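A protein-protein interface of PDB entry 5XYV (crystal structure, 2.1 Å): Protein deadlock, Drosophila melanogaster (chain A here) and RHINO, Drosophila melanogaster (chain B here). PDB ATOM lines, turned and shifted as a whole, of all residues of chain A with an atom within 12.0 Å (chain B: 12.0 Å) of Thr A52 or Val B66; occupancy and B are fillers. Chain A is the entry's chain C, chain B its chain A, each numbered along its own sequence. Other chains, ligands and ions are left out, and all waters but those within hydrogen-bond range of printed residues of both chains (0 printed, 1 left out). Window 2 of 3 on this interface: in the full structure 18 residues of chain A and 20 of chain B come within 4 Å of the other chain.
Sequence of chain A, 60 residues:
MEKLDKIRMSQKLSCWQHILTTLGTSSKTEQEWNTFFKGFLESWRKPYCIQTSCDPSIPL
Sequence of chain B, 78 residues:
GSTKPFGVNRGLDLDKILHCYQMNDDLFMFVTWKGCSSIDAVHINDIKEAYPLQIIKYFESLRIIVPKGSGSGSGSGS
Among the printed residues, pairs that only touch across the chains: Tyr A48 with Leu B62, Cys A49 with Arg B63, Cys A49 with Ile B65, Ile A50 with Phe B59, Ile A50 with Leu B62, Ile A50 with Ile B64 and Thr A52 with Ile B65.
Thr A52 touches two residues of chain B. Val B66 touches just one residue of chain A: Thr A52. No residue of chain A comes within 4 Å of Pro B67. Printed residues of chain A within 4 Å of Arg B63: Cys A49 (3.5 Å) and Ile A50 (3.2 Å). Of the printed residues of chain A, Phe B59 touches Ile A50. Of the printed residues of chain B, Cys A49 touches Arg B63 and Ile B65. Of the printed residues of chain A, Leu B62 touches Tyr A48 (3.0 Å) and Ile A50 (3.4 Å). Printed residues of chain B within 4 Å of Ile A50: Phe B59, Leu B62, Arg B63, Ile B64 and Ile B65. Gln B22 touches none of the printed residues of chain A. The nearest residue of chain A that does not touch Val B66 is Ile A50 (5.9 Å).
Of the 6 printed residues of chain A, 4 touch a printed residue of chain B. Printed residues of chain A that touch a printed residue of chain B: Tyr A48, Cys A49, Ile A50 and Thr A52. Of the 8 printed residues of chain B, 6 touch a printed residue of chain A. Printed residues of chain B that touch a printed residue of chain A: Phe B59, Leu B62, Arg B63, Ile B64, Ile B65 and Val B66.
N of Ile A50 is in hydrogen-bond range of O of Arg B63, at 3.2 Å. N of Ile B65 sits at hydrogen-bond distance from O of Ile A50, at 3.4 Å. The backbone carbonyl oxygen of Val B66 sits at hydrogen-bond distance from the side-chain hydroxyl of Thr A52 (3.4 Å).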
ATOM      1  N   TYR A  48     -18.006  -5.643   5.597  1.00  0.00           N
ATOM      2  CA  TYR A  48     -17.867  -5.364   4.172  1.00  0.00           C
ATOM      3  C   TYR A  48     -19.024  -4.564   3.589  1.00  0.00           C
ATOM      4  O   TYR A  48     -20.158  -4.644   4.050  1.00  0.00           O
ATOM      5  CB  TYR A  48     -17.693  -6.665   3.380  1.00  0.00           C
ATOM      6  CG  TYR A  48     -18.241  -7.897   4.062  1.00  0.00           C
ATOM      7  CD1 TYR A  48     -19.571  -8.256   3.926  1.00  0.00           C
ATOM      8  CD2 TYR A  48     -17.409  -8.725   4.809  1.00  0.00           C
ATOM      9  CE1 TYR A  48     -20.062  -9.370   4.553  1.00  0.00           C
ATOM     10  CE2 TYR A  48     -17.897  -9.860   5.428  1.00  0.00           C
ATOM     11  CZ  TYR A  48     -19.226 -10.181   5.289  1.00  0.00           C
ATOM     12  OH  TYR A  48     -19.708 -11.314   5.903  1.00  0.00           O
ATOM     13  N   CYS A  49     -18.704  -3.754   2.588  1.00  0.00           N
ATOM     14  CA  CYS A  49     -19.705  -3.127   1.740  1.00  0.00           C
ATOM     15  C   CYS A  49     -19.488  -3.610   0.317  1.00  0.00           C
ATOM     16  O   CYS A  49     -18.346  -3.754  -0.123  1.00  0.00           O
ATOM     17  CB  CYS A  49     -19.618  -1.599   1.799  1.00  0.00           C
ATOM     18  SG  CYS A  49     -19.269  -0.907   3.427  1.00  0.00           S
ATOM     19  N   ILE A  50     -20.574  -3.891  -0.395  1.00  0.00           N
ATOM     20  CA  ILE A  50     -20.484  -4.154  -1.829  1.00  0.00           C
ATOM     21  C   ILE A  50     -20.769  -2.835  -2.567  1.00  0.00           C
ATOM     22  O   ILE A  50     -21.776  -2.163  -2.307  1.00  0.00           O
ATOM     23  CB  ILE A  50     -21.464  -5.258  -2.273  1.00  0.00           C
ATOM     24  CG1 ILE A  50     -21.160  -6.560  -1.531  1.00  0.00           C
ATOM     25  CG2 ILE A  50     -21.337  -5.500  -3.754  1.00  0.00           C
ATOM     26  CD1 ILE A  50     -21.718  -7.796  -2.217  1.00  0.00           C
ATOM     27  N   GLN A  51     -19.875  -2.460  -3.473  1.00  0.00           N
ATOM     28  CA  GLN A  51     -19.892  -1.124  -4.056  1.00  0.00           C
ATOM     29  C   GLN A  51     -20.303  -1.155  -5.532  1.00  0.00           C
ATOM     30  O   GLN A  51     -19.558  -1.667  -6.378  1.00  0.00           O
ATOM     31  CB  GLN A  51     -18.510  -0.474  -3.879  1.00  0.00           C
ATOM     32  CG  GLN A  51     -18.179   0.653  -4.855  1.00  0.00           C
ATOM     33  CD  GLN A  51     -16.686   0.968  -4.912  1.00  0.00           C
ATOM     34  OE1 GLN A  51     -16.054   1.203  -3.883  1.00  0.00           O
ATOM     35  NE2 GLN A  51     -16.118   0.960  -6.118  1.00  0.00           N
ATOM     36  N   THR A  52     -21.498  -0.633  -5.837  1.00  0.00           N
ATOM     37  CA  THR A  52     -21.916  -0.479  -7.232  1.00  0.00           C
ATOM     38  C   THR A  52     -20.929   0.504  -7.861  1.00  0.00           C
ATOM     39  O   THR A  52     -20.811   1.663  -7.444  1.00  0.00           O
ATOM     40  CB  THR A  52     -23.388  -0.019  -7.379  1.00  0.00           C
ATOM     41  OG1 THR A  52     -23.723   0.895  -6.330  1.00  0.00           O
ATOM     42  CG2 THR A  52     -24.329  -1.222  -7.312  1.00  0.00           C
ATOM     43  N   SER A  53     -20.236   0.000  -8.876  1.00  0.00           N
ATOM     44  CA  SER A  53     -18.845   0.345  -9.167  1.00  0.00           C
ATOM     45  C   SER A  53     -18.593   1.779  -9.649  1.00  0.00           C
ATOM     46  O   SER A  53     -17.493   2.101 -10.107  1.00  0.00           O
ATOM     47  CB  SER A  53     -18.321  -0.654 -10.204  1.00  0.00           C
ATOM     48  OG  SER A  53     -17.976  -1.927  -9.597  1.00  0.00           O
ATOM     49  N   GLN B  22     -12.069 -11.016  -2.245  1.00  0.00           N
ATOM     50  CA  GLN B  22     -11.925 -10.774  -3.671  1.00  0.00           C
ATOM     51  C   GLN B  22     -10.499 -10.364  -3.986  1.00  0.00           C
ATOM     52  O   GLN B  22      -9.979  -9.445  -3.369  1.00  0.00           O
ATOM     53  CB  GLN B  22     -12.908  -9.690  -4.096  1.00  0.00           C
ATOM     54  CG  GLN B  22     -12.943  -9.323  -5.561  1.00  0.00           C
ATOM     55  CD  GLN B  22     -13.941  -8.198  -5.800  1.00  0.00           C
ATOM     56  OE1 GLN B  22     -13.785  -7.097  -5.269  1.00  0.00           O
ATOM     57  NE2 GLN B  22     -14.989  -8.485  -6.565  1.00  0.00           N
ATOM     58  N   PHE B  59     -24.669 -12.978  -0.584  1.00  0.00           N
ATOM     59  CA  PHE B  59     -24.505 -11.610  -1.073  1.00  0.00           C
ATOM     60  C   PHE B  59     -25.628 -10.688  -0.596  1.00  0.00           C
ATOM     61  O   PHE B  59     -25.386  -9.524  -0.324  1.00  0.00           O
ATOM     62  CB  PHE B  59     -24.456 -11.566  -2.590  1.00  0.00           C
ATOM     63  CG  PHE B  59     -23.153 -12.001  -3.169  1.00  0.00           C
ATOM     64  CD1 PHE B  59     -21.982 -11.332  -2.845  1.00  0.00           C
ATOM     65  CD2 PHE B  59     -23.099 -13.038  -4.076  1.00  0.00           C
ATOM     66  CE1 PHE B  59     -20.769 -11.714  -3.388  1.00  0.00           C
ATOM     67  CE2 PHE B  59     -21.883 -13.441  -4.625  1.00  0.00           C
ATOM     68  CZ  PHE B  59     -20.718 -12.774  -4.282  1.00  0.00           C
ATOM     69  N   LEU B  62     -25.104  -8.955   2.682  1.00  0.00           N
ATOM     70  CA  LEU B  62     -24.130  -7.877   2.770  1.00  0.00           C
ATOM     71  C   LEU B  62     -24.837  -6.548   2.564  1.00  0.00           C
ATOM     72  O   LEU B  62     -25.920  -6.496   1.974  1.00  0.00           O
ATOM     73  CB  LEU B  62     -23.015  -8.033   1.728  1.00  0.00           C
ATOM     74  CG  LEU B  62     -22.369  -9.393   1.456  1.00  0.00           C
ATOM     75  CD1 LEU B  62     -21.012  -9.239   0.784  1.00  0.00           C
ATOM     76  CD2 LEU B  62     -22.278 -10.255   2.674  1.00  0.00           C
ATOM     77  N   ARG B  63     -24.239  -5.463   3.031  1.00  0.00           N
ATOM     78  CA  ARG B  63     -24.869  -4.178   2.783  1.00  0.00           C
ATOM     79  C   ARG B  63     -24.345  -3.544   1.504  1.00  0.00           C
ATOM     80  O   ARG B  63     -23.165  -3.220   1.384  1.00  0.00           O
ATOM     81  CB  ARG B  63     -24.702  -3.252   3.984  1.00  0.00           C
ATOM     82  CG  ARG B  63     -25.716  -3.604   5.069  1.00  0.00           C
ATOM     83  CD  ARG B  63     -27.130  -3.553   4.474  1.00  0.00           C
ATOM     84  NE  ARG B  63     -27.892  -4.783   4.702  1.00  0.00           N
ATOM     85  CZ  ARG B  63     -29.012  -4.843   5.418  1.00  0.00           C
ATOM     86  NH1 ARG B  63     -29.506  -3.740   5.963  1.00  0.00           N
ATOM     87  NH2 ARG B  63     -29.643  -6.000   5.578  1.00  0.00           N
ATOM     88  N   ILE B  64     -25.257  -3.402   0.543  1.00  0.00           N
ATOM     89  CA  ILE B  64     -24.963  -2.841  -0.769  1.00  0.00           C
ATOM     90  C   ILE B  64     -25.283  -1.357  -0.757  1.00  0.00           C
ATOM     91  O   ILE B  64     -26.456  -0.953  -0.807  1.00  0.00           O
ATOM     92  CB  ILE B  64     -25.766  -3.551  -1.873  1.00  0.00           C
ATOM     93  CG1 ILE B  64     -25.658  -5.067  -1.691  1.00  0.00           C
ATOM     94  CG2 ILE B  64     -25.274  -3.126  -3.247  1.00  0.00           C
ATOM     95  CD1 ILE B  64     -26.463  -5.864  -2.667  1.00  0.00           C
ATOM     96  N   ILE B  65     -24.224  -0.556  -0.673  1.00  0.00           N
ATOM     97  CA  ILE B  65     -24.333   0.882  -0.466  1.00  0.00           C
ATOM     98  C   ILE B  65     -24.240   1.674  -1.779  1.00  0.00           C
ATOM     99  O   ILE B  65     -23.921   1.125  -2.836  1.00  0.00           O
ATOM    100  CB  ILE B  65     -23.248   1.368   0.531  1.00  0.00           C
ATOM    101  CG1 ILE B  65     -21.901   0.702   0.229  1.00  0.00           C
ATOM    102  CG2 ILE B  65     -23.647   1.032   1.959  1.00  0.00           C
ATOM    103  CD1 ILE B  65     -20.988   1.492  -0.700  1.00  0.00           C
ATOM    104  N   VAL B  66     -24.510   2.972  -1.686  1.00  0.00           N
ATOM    105  CA  VAL B  66     -24.768   3.809  -2.858  1.00  0.00           C
ATOM    106  C   VAL B  66     -23.548   4.156  -3.746  1.00  0.00           C
ATOM    107  O   VAL B  66     -23.631   4.023  -4.969  1.00  0.00           O
ATOM    108  CB  VAL B  66     -25.476   5.118  -2.414  1.00  0.00           C
ATOM    109  CG1 VAL B  66     -25.592   6.097  -3.568  1.00  0.00           C
ATOM    110  CG2 VAL B  66     -26.854   4.801  -1.829  1.00  0.00           C
ATOM    111  N   PRO B  67     -22.411   4.584  -3.161  1.00  0.00           N
ATOM    112  CA  PRO B  67     -21.995   4.821  -1.770  1.00  0.00           C
ATOM    113  C   PRO B  67     -22.558   6.106  -1.173  1.00  0.00           C
ATOM    114  O   PRO B  67     -21.783   7.031  -0.927  1.00  0.00           O
ATOM    115  CB  PRO B  67     -20.462   4.913  -1.869  1.00  0.00           C
ATOM    116  CG  PRO B  67     -20.109   4.388  -3.237  1.00  0.00           C
ATOM    117  CD  PRO B  67     -21.277   4.745  -4.087  1.00  0.00           C
